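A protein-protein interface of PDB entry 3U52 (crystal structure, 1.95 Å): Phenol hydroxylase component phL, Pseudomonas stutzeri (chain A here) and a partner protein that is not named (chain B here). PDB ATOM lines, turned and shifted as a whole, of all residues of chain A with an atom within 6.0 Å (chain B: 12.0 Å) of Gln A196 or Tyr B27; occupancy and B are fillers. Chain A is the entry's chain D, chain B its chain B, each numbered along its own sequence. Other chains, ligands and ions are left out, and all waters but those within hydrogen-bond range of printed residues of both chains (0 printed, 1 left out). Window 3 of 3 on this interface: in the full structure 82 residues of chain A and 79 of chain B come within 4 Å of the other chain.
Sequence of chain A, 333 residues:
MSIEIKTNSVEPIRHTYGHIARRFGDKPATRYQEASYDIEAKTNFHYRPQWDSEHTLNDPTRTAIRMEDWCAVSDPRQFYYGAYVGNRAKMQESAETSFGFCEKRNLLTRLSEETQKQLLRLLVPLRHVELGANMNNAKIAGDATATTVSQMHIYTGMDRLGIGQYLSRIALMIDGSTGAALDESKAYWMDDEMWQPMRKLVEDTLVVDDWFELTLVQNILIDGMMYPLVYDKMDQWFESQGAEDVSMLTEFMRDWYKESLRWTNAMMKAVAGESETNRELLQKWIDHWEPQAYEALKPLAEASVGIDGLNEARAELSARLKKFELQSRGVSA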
ATOM      1  N   TYR A 188      20.975 -17.104  18.187  1.00  0.00           N
ATOM      2  CA  TYR A 188      20.539 -18.529  18.295  1.00  0.00           C
ATOM      3  C   TYR A 188      19.206 -18.695  19.084  1.00  0.00           C
ATOM      4  O   TYR A 188      18.281 -19.365  18.643  1.00  0.00           O
ATOM      5  CB  TYR A 188      21.643 -19.431  18.904  1.00  0.00           C
ATOM      6  CG  TYR A 188      22.926 -19.479  18.103  1.00  0.00           C
ATOM      7  CD1 TYR A 188      24.152 -19.188  18.686  1.00  0.00           C
ATOM      8  CD2 TYR A 188      22.902 -19.799  16.746  1.00  0.00           C
ATOM      9  CE1 TYR A 188      25.332 -19.221  17.950  1.00  0.00           C
ATOM     10  CE2 TYR A 188      24.058 -19.837  15.993  1.00  0.00           C
ATOM     11  CZ  TYR A 188      25.272 -19.532  16.601  1.00  0.00           C
ATOM     12  OH  TYR A 188      26.404 -19.554  15.832  1.00  0.00           O
ATOM     13  N   TRP A 189      19.135 -18.077  20.259  1.00  0.00           N
ATOM     14  CA  TRP A 189      17.936 -18.066  21.097  1.00  0.00           C
ATOM     15  C   TRP A 189      16.704 -17.617  20.308  1.00  0.00           C
ATOM     16  O   TRP A 189      15.645 -18.264  20.404  1.00  0.00           O
ATOM     17  CB  TRP A 189      18.177 -17.150  22.303  1.00  0.00           C
ATOM     18  CG  TRP A 189      17.063 -16.936  23.200  1.00  0.00           C
ATOM     19  CD1 TRP A 189      16.365 -15.763  23.370  1.00  0.00           C
ATOM     20  CD2 TRP A 189      16.489 -17.886  24.091  1.00  0.00           C
ATOM     21  NE1 TRP A 189      15.380 -15.939  24.325  1.00  0.00           N
ATOM     22  CE2 TRP A 189      15.429 -17.237  24.771  1.00  0.00           C
ATOM     23  CE3 TRP A 189      16.761 -19.244  24.386  1.00  0.00           C
ATOM     24  CZ2 TRP A 189      14.675 -17.874  25.762  1.00  0.00           C
ATOM     25  CZ3 TRP A 189      15.974 -19.887  25.358  1.00  0.00           C
ATOM     26  CH2 TRP A 189      14.935 -19.213  26.007  1.00  0.00           C
ATOM     27  N   MET A 190      16.853 -16.553  19.537  1.00  0.00           N
ATOM     28  CA  MET A 190      15.726 -15.904  18.831  1.00  0.00           C
ATOM     29  C   MET A 190      15.315 -16.630  17.522  1.00  0.00           C
ATOM     30  O   MET A 190      14.111 -16.747  17.219  1.00  0.00           O
ATOM     31  CB  MET A 190      16.030 -14.449  18.511  1.00  0.00           C
ATOM     32  CG  MET A 190      16.095 -13.483  19.726  1.00  0.00           C
ATOM     33  SD  MET A 190      14.614 -13.469  20.734  1.00  0.00           S
ATOM     34  CE  MET A 190      13.472 -12.512  19.710  1.00  0.00           C
ATOM     35  N   ASP A 191      16.309 -17.131  16.797  1.00  0.00           N
ATOM     36  CA  ASP A 191      16.114 -17.646  15.423  1.00  0.00           C
ATOM     37  C   ASP A 191      16.501 -19.096  15.130  1.00  0.00           C
ATOM     38  O   ASP A 191      16.049 -19.640  14.138  1.00  0.00           O
ATOM     39  CB  ASP A 191      16.825 -16.736  14.434  1.00  0.00           C
ATOM     40  CG  ASP A 191      16.309 -15.305  14.482  1.00  0.00           C
ATOM     41  OD1 ASP A 191      15.076 -15.088  14.645  1.00  0.00           O
ATOM     42  OD2 ASP A 191      17.145 -14.378  14.370  1.00  0.00           O
ATOM     43  N   ASP A 192      17.349 -19.728  15.950  1.00  0.00           N
ATOM     44  CA  ASP A 192      17.683 -21.135  15.716  1.00  0.00           C
ATOM     45  C   ASP A 192      16.510 -22.009  16.133  1.00  0.00           C
ATOM     46  O   ASP A 192      16.023 -21.924  17.258  1.00  0.00           O
ATOM     47  CB  ASP A 192      18.953 -21.565  16.469  1.00  0.00           C
ATOM     48  CG  ASP A 192      19.441 -22.966  16.065  1.00  0.00           C
ATOM     49  OD1 ASP A 192      18.621 -23.893  15.860  1.00  0.00           O
ATOM     50  OD2 ASP A 192      20.667 -23.148  15.946  1.00  0.00           O
ATOM     51  N   GLU A 193      16.077 -22.891  15.235  1.00  0.00           N
ATOM     52  CA  GLU A 193      14.941 -23.765  15.519  1.00  0.00           C
ATOM     53  C   GLU A 193      15.151 -24.636  16.767  1.00  0.00           C
ATOM     54  O   GLU A 193      14.198 -24.972  17.437  1.00  0.00           O
ATOM     55  CB  GLU A 193      14.586 -24.616  14.274  1.00  0.00           C
ATOM     56  CG  GLU A 193      15.762 -25.513  13.804  1.00  0.00           C
ATOM     57  CD  GLU A 193      15.411 -26.377  12.579  1.00  0.00           C
ATOM     58  OE1 GLU A 193      15.205 -27.611  12.761  1.00  0.00           O
ATOM     59  OE2 GLU A 193      15.329 -25.810  11.454  1.00  0.00           O
ATOM     60  N   MET A 194      16.398 -24.980  17.062  1.00  0.00           N
ATOM     61  CA  MET A 194      16.787 -25.779  18.223  1.00  0.00           C
ATOM     62  C   MET A 194      16.283 -25.144  19.525  1.00  0.00           C
ATOM     63  O   MET A 194      15.875 -25.878  20.440  1.00  0.00           O
ATOM     64  CB  MET A 194      18.311 -25.839  18.292  1.00  0.00           C
ATOM     65  CG  MET A 194      18.915 -27.030  19.064  1.00  0.00           C
ATOM     66  SD  MET A 194      20.562 -26.564  19.709  1.00  0.00           S
ATOM     67  CE  MET A 194      19.998 -25.895  21.256  1.00  0.00           C
ATOM     68  N   TRP A 195      16.320 -23.798  19.621  1.00  0.00           N
ATOM     69  CA  TRP A 195      15.908 -23.095  20.856  1.00  0.00           C
ATOM     70  C   TRP A 195      14.436 -22.764  20.930  1.00  0.00           C
ATOM     71  O   TRP A 195      13.960 -22.301  21.991  1.00  0.00           O
ATOM     72  CB  TRP A 195      16.741 -21.813  21.103  1.00  0.00           C
ATOM     73  CG  TRP A 195      18.085 -22.187  21.504  1.00  0.00           C
ATOM     74  CD1 TRP A 195      19.187 -22.257  20.709  1.00  0.00           C
ATOM     75  CD2 TRP A 195      18.485 -22.655  22.804  1.00  0.00           C
ATOM     76  NE1 TRP A 195      20.280 -22.715  21.453  1.00  0.00           N
ATOM     77  CE2 TRP A 195      19.862 -22.981  22.731  1.00  0.00           C
ATOM     78  CE3 TRP A 195      17.810 -22.823  24.023  1.00  0.00           C
ATOM     79  CZ2 TRP A 195      20.578 -23.482  23.833  1.00  0.00           C
ATOM     80  CZ3 TRP A 195      18.516 -23.308  25.121  1.00  0.00           C
ATOM     81  CH2 TRP A 195      19.895 -23.620  25.018  1.00  0.00           C
ATOM     82  N   GLN A 196      13.702 -22.924  19.817  1.00  0.00           N
ATOM     83  CA  GLN A 196      12.329 -22.389  19.814  1.00  0.00           C
ATOM     84  C   GLN A 196      11.372 -23.077  20.785  1.00  0.00           C
ATOM     85  O   GLN A 196      10.581 -22.402  21.426  1.00  0.00           O
ATOM     86  CB  GLN A 196      11.743 -22.192  18.399  1.00  0.00           C
ATOM     87  CG  GLN A 196      12.570 -21.217  17.569  1.00  0.00           C
ATOM     88  CD  GLN A 196      13.122 -20.022  18.391  1.00  0.00           C
ATOM     89  OE1 GLN A 196      12.370 -19.183  18.887  1.00  0.00           O
ATOM     90  NE2 GLN A 196      14.449 -19.945  18.501  1.00  0.00           N
ATOM     91  N   PRO A 197      11.438 -24.411  20.922  1.00  0.00           N
ATOM     92  CA  PRO A 197      10.576 -25.029  21.930  1.00  0.00           C
ATOM     93  C   PRO A 197      10.884 -24.503  23.354  1.00  0.00           C
ATOM     94  O   PRO A 197       9.966 -24.311  24.168  1.00  0.00           O
ATOM     95  CB  PRO A 197      10.926 -26.503  21.825  1.00  0.00           C
ATOM     96  CG  PRO A 197      11.337 -26.668  20.342  1.00  0.00           C
ATOM     97  CD  PRO A 197      12.154 -25.416  20.124  1.00  0.00           C
ATOM     98  N   MET A 198      12.155 -24.259  23.636  1.00  0.00           N
ATOM     99  CA  MET A 198      12.496 -23.749  24.992  1.00  0.00           C
ATOM    100  C   MET A 198      11.999 -22.331  25.158  1.00  0.00           C
ATOM    101  O   MET A 198      11.387 -21.993  26.157  1.00  0.00           O
ATOM    102  CB  MET A 198      13.972 -23.859  25.271  1.00  0.00           C
ATOM    103  CG  MET A 198      14.379 -23.232  26.629  1.00  0.00           C
ATOM    104  SD  MET A 198      13.825 -24.215  28.060  1.00  0.00           S
ATOM    105  CE  MET A 198      15.150 -25.409  28.166  1.00  0.00           C
ATOM    106  N   ARG A 199      12.239 -21.498  24.148  1.00  0.00           N
ATOM    107  CA  ARG A 199      11.889 -20.115  24.249  1.00  0.00           C
ATOM    108  C   ARG A 199      10.373 -19.942  24.395  1.00  0.00           C
ATOM    109  O   ARG A 199       9.914 -19.120  25.195  1.00  0.00           O
ATOM    110  CB  ARG A 199      12.405 -19.424  23.023  1.00  0.00           C
ATOM    111  CG  ARG A 199      12.454 -17.996  23.169  1.00  0.00           C
ATOM    112  CD  ARG A 199      12.977 -17.407  21.884  1.00  0.00           C
ATOM    113  NE  ARG A 199      12.074 -16.343  21.796  1.00  0.00           N
ATOM    114  CZ  ARG A 199      11.565 -15.808  20.731  1.00  0.00           C
ATOM    115  NH1 ARG A 199      11.881 -16.166  19.487  1.00  0.00           N
ATOM    116  NH2 ARG A 199      10.715 -14.872  21.006  1.00  0.00           N
ATOM    117  N   LYS A 200       9.604 -20.718  23.612  1.00  0.00           N
ATOM    118  CA  LYS A 200       8.146 -20.747  23.730  1.00  0.00           C
ATOM    119  C   LYS A 200       7.697 -21.211  25.119  1.00  0.00           C
ATOM    120  O   LYS A 200       6.766 -20.637  25.699  1.00  0.00           O
ATOM    121  CB  LYS A 200       7.499 -21.675  22.656  1.00  0.00           C
ATOM    122  CG  LYS A 200       5.931 -21.777  22.849  1.00  0.00           C
ATOM    123  CD  LYS A 200       5.237 -22.549  21.717  1.00  0.00           C
ATOM    124  CE  LYS A 200       3.778 -22.868  22.027  1.00  0.00           C
ATOM    125  NZ  LYS A 200       3.015 -21.693  22.572  1.00  0.00           N
ATOM    126  N   LEU A 201       8.328 -22.266  25.640  1.00  0.00           N
ATOM    127  CA  LEU A 201       7.982 -22.751  26.974  1.00  0.00           C
ATOM    128  C   LEU A 201       8.270 -21.657  28.030  1.00  0.00           C
ATOM    129  O   LEU A 201       7.410 -21.384  28.904  1.00  0.00           O
ATOM    130  CB  LEU A 201       8.732 -24.038  27.326  1.00  0.00           C
ATOM    131  CG  LEU A 201       8.786 -24.415  28.820  1.00  0.00           C
ATOM    132  CD1 LEU A 201       7.362 -24.656  29.372  1.00  0.00           C
ATOM    133  CD2 LEU A 201       9.705 -25.601  29.050  1.00  0.00           C
ATOM    134  N   GLU A 203       8.465 -18.367  27.613  1.00  0.00           N
ATOM    135  CA  GLU A 203       7.425 -17.352  27.451  1.00  0.00           C
ATOM    136  C   GLU A 203       6.030 -17.767  28.002  1.00  0.00           C
ATOM    137  O   GLU A 203       5.304 -16.935  28.612  1.00  0.00           O
ATOM    138  CB  GLU A 203       7.348 -16.855  25.990  1.00  0.00           C
ATOM    139  CG  GLU A 203       8.616 -16.179  25.526  1.00  0.00           C
ATOM    140  CD  GLU A 203       8.515 -15.624  24.128  1.00  0.00           C
ATOM    141  OE1 GLU A 203       9.564 -15.284  23.508  1.00  0.00           O
ATOM    142  OE2 GLU A 203       7.363 -15.511  23.660  1.00  0.00           O
ATOM    143  N   ASP A 204       5.690 -19.047  27.848  1.00  0.00           N
ATOM    144  CA  ASP A 204       4.450 -19.615  28.419  1.00  0.00           C
ATOM    145  C   ASP A 204       4.410 -19.556  29.964  1.00  0.00           C
ATOM    146  O   ASP A 204       3.401 -19.167  30.572  1.00  0.00           O
ATOM    147  CB  ASP A 204       4.234 -21.046  27.933  1.00  0.00           C
ATOM    148  CG  ASP A 204       3.785 -21.138  26.438  1.00  0.00           C
ATOM    149  OD1 ASP A 204       3.467 -20.105  25.749  1.00  0.00           O
ATOM    150  OD2 ASP A 204       3.794 -22.289  25.946  1.00  0.00           O
ATOM    151  N   TRP B  23      14.599 -10.442  26.211  1.00  0.00           N
ATOM    152  CA  TRP B  23      14.356 -10.486  24.767  1.00  0.00           C
ATOM    153  C   TRP B  23      12.930 -10.040  24.444  1.00  0.00           C
ATOM    154  O   TRP B  23      12.065  -9.978  25.336  1.00  0.00           O
ATOM    155  CB  TRP B  23      14.628 -11.897  24.170  1.00  0.00           C
ATOM    156  CG  TRP B  23      13.646 -12.914  24.644  1.00  0.00           C
ATOM    157  CD1 TRP B  23      12.519 -13.315  24.008  1.00  0.00           C
ATOM    158  CD2 TRP B  23      13.686 -13.629  25.885  1.00  0.00           C
ATOM    159  NE1 TRP B  23      11.856 -14.256  24.756  1.00  0.00           N
ATOM    160  CE2 TRP B  23      12.544 -14.460  25.924  1.00  0.00           C
ATOM    161  CE3 TRP B  23      14.580 -13.653  26.974  1.00  0.00           C
ATOM    162  CZ2 TRP B  23      12.254 -15.294  27.018  1.00  0.00           C
ATOM    163  CZ3 TRP B  23      14.307 -14.500  28.048  1.00  0.00           C
ATOM    164  CH2 TRP B  23      13.132 -15.310  28.060  1.00  0.00           C
ATOM    165  N   GLU B  24      12.707  -9.725  23.167  1.00  0.00           N
ATOM    166  CA  GLU B  24      11.371  -9.404  22.693  1.00  0.00           C
ATOM    167  C   GLU B  24      10.588 -10.709  22.489  1.00  0.00           C
ATOM    168  O   GLU B  24      11.048 -11.602  21.779  1.00  0.00           O
ATOM    169  CB  GLU B  24      11.431  -8.548  21.431  1.00  0.00           C
ATOM    170  CG  GLU B  24      11.898  -7.117  21.724  1.00  0.00           C
ATOM    171  CD  GLU B  24      10.810  -6.224  22.362  1.00  0.00           C
ATOM    172  OE1 GLU B  24      11.163  -5.125  22.867  1.00  0.00           O
ATOM    173  OE2 GLU B  24       9.613  -6.601  22.345  1.00  0.00           O
ATOM    174  N   PRO B  25       9.456 -10.869  23.192  1.00  0.00           N
ATOM    175  CA  PRO B  25       8.754 -12.143  23.085  1.00  0.00           C
ATOM    176  C   PRO B  25       8.085 -12.362  21.711  1.00  0.00           C
ATOM    177  O   PRO B  25       7.704 -11.388  21.061  1.00  0.00           O
ATOM    178  CB  PRO B  25       7.723 -12.085  24.211  1.00  0.00           C
ATOM    179  CG  PRO B  25       7.573 -10.647  24.555  1.00  0.00           C
ATOM    180  CD  PRO B  25       8.825  -9.954  24.164  1.00  0.00           C
ATOM    181  N   THR B  26       7.929 -13.631  21.326  1.00  0.00           N
ATOM    182  CA  THR B  26       7.382 -14.029  20.016  1.00  0.00           C
ATOM    183  C   THR B  26       6.103 -14.856  20.221  1.00  0.00           C
ATOM    184  O   THR B  26       5.151 -14.725  19.447  1.00  0.00           O
ATOM    185  CB  THR B  26       8.441 -14.821  19.190  1.00  0.00           C
ATOM    186  OG1 THR B  26       9.600 -13.996  18.964  1.00  0.00           O
ATOM    187  CG2 THR B  26       7.912 -15.277  17.832  1.00  0.00           C
ATOM    188  N   TYR B  27       6.055 -15.643  21.294  1.00  0.00           N
ATOM    189  CA  TYR B  27       5.036 -16.682  21.505  1.00  0.00           C
ATOM    190  C   TYR B  27       3.929 -16.269  22.435  1.00  0.00           C
ATOM    191  O   TYR B  27       2.861 -16.888  22.454  1.00  0.00           O
ATOM    192  CB  TYR B  27       5.701 -17.963  22.017  1.00  0.00           C
ATOM    193  CG  TYR B  27       6.786 -18.373  21.068  1.00  0.00           C
ATOM    194  CD1 TYR B  27       8.127 -18.129  21.351  1.00  0.00           C
ATOM    195  CD2 TYR B  27       6.459 -18.951  19.822  1.00  0.00           C
ATOM    196  CE1 TYR B  27       9.133 -18.491  20.444  1.00  0.00           C
ATOM    197  CE2 TYR B  27       7.444 -19.307  18.908  1.00  0.00           C
ATOM    198  CZ  TYR B  27       8.771 -19.074  19.215  1.00  0.00           C
ATOM    199  OH  TYR B  27       9.727 -19.456  18.290  1.00  0.00           O
ATOM    200  N   GLN B  28       4.188 -15.234  23.224  1.00  0.00           N
ATOM    201  CA  GLN B  28       3.166 -14.603  24.030  1.00  0.00           C
ATOM    202  C   GLN B  28       3.291 -13.137  23.719  1.00  0.00           C
ATOM    203  O   GLN B  28       4.363 -12.709  23.351  1.00  0.00           O
ATOM    204  CB  GLN B  28       3.385 -14.840  25.522  1.00  0.00           C
ATOM    205  CG  GLN B  28       3.343 -16.279  25.939  1.00  0.00           C
ATOM    206  CD  GLN B  28       1.923 -16.823  26.097  1.00  0.00           C
ATOM    207  OE1 GLN B  28       1.720 -18.036  26.063  1.00  0.00           O
ATOM    208  NE2 GLN B  28       0.946 -15.933  26.282  1.00  0.00           N
ATOM    209  N   ASP B  29       2.206 -12.369  23.844  1.00  0.00           N
ATOM    210  CA  ASP B  29       2.274 -10.931  23.601  1.00  0.00           C
ATOM    211  C   ASP B  29       2.921 -10.265  24.824  1.00  0.00           C
ATOM    212  O   ASP B  29       2.687 -10.674  25.977  1.00  0.00           O
ATOM    213  CB  ASP B  29       0.869 -10.315  23.394  1.00  0.00           C
ATOM    214  CG  ASP B  29      -0.002 -11.073  22.348  1.00  0.00           C
ATOM    215  OD1 ASP B  29       0.521 -11.792  21.429  1.00  0.00           O
ATOM    216  OD2 ASP B  29      -1.254 -10.911  22.433  1.00  0.00           O
ATOM    217  N   LYS B  30       3.700  -9.216  24.584  1.00  0.00           N
ATOM    218  CA  LYS B  30       4.361  -8.483  25.646  1.00  0.00           C
ATOM    219  C   LYS B  30       3.385  -8.018  26.708  1.00  0.00           C
ATOM    220  O   LYS B  30       3.698  -8.019  27.898  1.00  0.00           O
ATOM    221  CB  LYS B  30       5.128  -7.275  25.081  1.00  0.00           C
ATOM    222  CG  LYS B  30       6.473  -7.056  25.751  1.00  0.00           C
ATOM    223  CD  LYS B  30       7.241  -5.884  25.154  1.00  0.00           C
ATOM    224  CE  LYS B  30       8.689  -5.918  25.661  1.00  0.00           C
ATOM    225  NZ  LYS B  30       9.376  -4.577  25.604  1.00  0.00           N
ATOM    226  N   LYS B  31       2.183  -7.634  26.281  1.00  0.00           N
ATOM    227  CA  LYS B  31       1.188  -7.091  27.205  1.00  0.00           C
ATOM    228  C   LYS B  31       0.596  -8.134  28.138  1.00  0.00           C
ATOM    229  O   LYS B  31       0.103  -7.783  29.190  1.00  0.00           O
ATOM    230  CB  LYS B  31       0.084  -6.316  26.485  1.00  0.00           C
ATOM    231  CG  LYS B  31       0.573  -5.029  25.828  1.00  0.00           C
ATOM    232  CD  LYS B  31       1.167  -4.043  26.869  1.00  0.00           C
ATOM    233  CE  LYS B  31       2.293  -3.175  26.300  1.00  0.00           C
ATOM    234  NZ  LYS B  31       2.858  -2.332  27.414  1.00  0.00           N
ATOM    235  N   ASP B  32       0.636  -9.406  27.764  1.00  0.00           N
ATOM    236  CA  ASP B  32       0.205 -10.475  28.667  1.00  0.00           C
ATOM    237  C   ASP B  32       1.320 -10.829  29.656  1.00  0.00           C
ATOM    238  O   ASP B  32       1.046 -11.148  30.798  1.00  0.00           O
ATOM    239  CB  ASP B  32      -0.174 -11.722  27.895  1.00  0.00           C
ATOM    240  CG  ASP B  32      -1.546 -11.586  27.165  1.00  0.00           C
ATOM    241  OD1 ASP B  32      -2.447 -10.850  27.660  1.00  0.00           O
ATOM    242  OD2 ASP B  32      -1.707 -12.236  26.105  1.00  0.00           O
ATOM    243  N   ILE B  33       2.564 -10.748  29.203  1.00  0.00           N
ATOM    244  CA  ILE B  33       3.727 -10.905  30.113  1.00  0.00           C
ATOM    245  C   ILE B  33       3.867  -9.734  31.107  1.00  0.00           C
ATOM    246  O   ILE B  33       4.200  -9.965  32.297  1.00  0.00           O
ATOM    247  CB  ILE B  33       5.026 -11.159  29.306  1.00  0.00           C
ATOM    248  CG1 ILE B  33       4.878 -12.480  28.581  1.00  0.00           C
ATOM    249  CG2 ILE B  33       6.335 -11.188  30.244  1.00  0.00           C
ATOM    250  CD1 ILE B  33       5.938 -12.740  27.530  1.00  0.00           C
ATOM    251  N   PHE B  34       3.600  -8.502  30.625  1.00  0.00           N
ATOM    252  CA  PHE B  34       3.727  -7.250  31.392  1.00  0.00           C
ATOM    253  C   PHE B  34       2.396  -6.441  31.402  1.00  0.00           C
ATOM    254  O   PHE B  34       2.310  -5.409  30.738  1.00  0.00           O
ATOM    255  CB  PHE B  34       4.877  -6.365  30.857  1.00  0.00           C
ATOM    256  CG  PHE B  34       6.239  -7.060  30.834  1.00  0.00           C
ATOM    257  CD1 PHE B  34       6.819  -7.448  29.614  1.00  0.00           C
ATOM    258  CD2 PHE B  34       6.921  -7.328  32.018  1.00  0.00           C
ATOM    259  CE1 PHE B  34       8.091  -8.087  29.575  1.00  0.00           C
ATOM    260  CE2 PHE B  34       8.191  -7.965  32.002  1.00  0.00           C
ATOM    261  CZ  PHE B  34       8.763  -8.351  30.789  1.00  0.00           C
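Among the printed residues, merely in contact across the chains: Trp A189 with Trp B23, Met A190 with Trp B23, Met A190 with Glu B24, Arg A199 with Trp B23, Arg A199 with Pro B25, Arg A199 with Tyr B27, Lys A200 with Tyr B27 and Glu A203 with Pro B25.
N of Gln B28 is in hydrogen-bond range of OE2 of Glu A203 (3.2 Å). The backbone NH (N) of Thr B26 lies within hydrogen-bond range of the side-chain carboxylate (OE2) of Glu A203 (3.0 Å). N of Tyr B27 sits at hydrogen-bond distance from OE2 of Glu A203, 2.7 Å away. NH2 of Arg A199 lies within hydrogen-bond range of O of Glu B24, 3.4 Å away. The guanidinium group (NH2) of Arg A199 lies within hydrogen-bond range of the side-chain hydroxyl (OG1) of Thr B26, 2.5 Å away. The side-chain hydroxyl (OH) of Tyr B27 lies within hydrogen-bond range of the side-chain amide oxygen (OE1) of Gln A196 (2.7 Å). The indole nitrogen (NE1) of Trp B23 lies within hydrogen-bond range of the side-chain carboxylate (OE1) of Glu A203, 2.8 Å away. The side-chain carboxylate of Asp A204 lies close to the side-chain amide oxygen of Gln B28 (2.7 Å).
O of Met A190 sits at hydrogen-bond distance from NH1 of Arg A199 (3.2 Å). OD2 of Asp A204 is in salt-bridge range of NZ of Lys A200. The backbone carbonyl oxygen of Trp A189 lies within hydrogen-bond range of the side-chain amide nitrogen of Gln A196. The side-chain amide oxygen (OE1) of Gln A196 lies close to the backbone carbonyl oxygen (O) of Met A190 (3.4 Å). The side-chain amide oxygen of Gln A196 is in hydrogen-bond range of the guanidinium group of Arg A199 (3.1 Å). OE1 of Glu A203 lies within salt-bridge range of NH2 of Arg A199 (2.8 Å).
Printed residues of chain B that touch a printed residue of chain A: Trp B23, Glu B24, Pro B25, Thr B26, Tyr B27 and Gln B28. Hydrophobic or aromatic side chains of chain B that line the printed part of chain A: Trp B23, Pro B25 and Tyr B27. Of the 16 printed residues of chain A, 7 touch a printed residue of chain B. Hydrophobic or aromatic side chains of chain A within 4 Å of the printed part of chain B: Trp A189 and Met A190.
Of chain B, only Trp B23 (3.3 Å) comes within 4 Å of Trp A189. Met A190 touches two residues of chain B. No residue of chain B comes within 4 Å of Asp A191. No residue of chain B comes within 4 Å of Asp A192. Gln A196 touches just one residue of chain B: Tyr B27 (2.7 Å). No residue of chain B comes within 4 Å of Pro A197. Printed residues of chain B within 4 Å of Arg A199: Trp B23, Glu B24, Pro B25, Thr B26 and Tyr B27. Of chain B, only Tyr B27 comes within 4 Å of Lys A200. Of the printed residues of chain A, Thr B26 touches Arg A199 and Glu A203. Tyr B27 touches just these residues of chain A: Gln A196 (2.7 Å), Arg A199 (3.6 Å), Lys A200 (3.5 Å) and Glu A203 (2.7 Å). Printed residues of chain A within 4 Å of Gln B28: Glu A203 and Asp A204. The nearest residue of chain B that does not touch Gln A196 is Thr B26 (5.9 Å).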
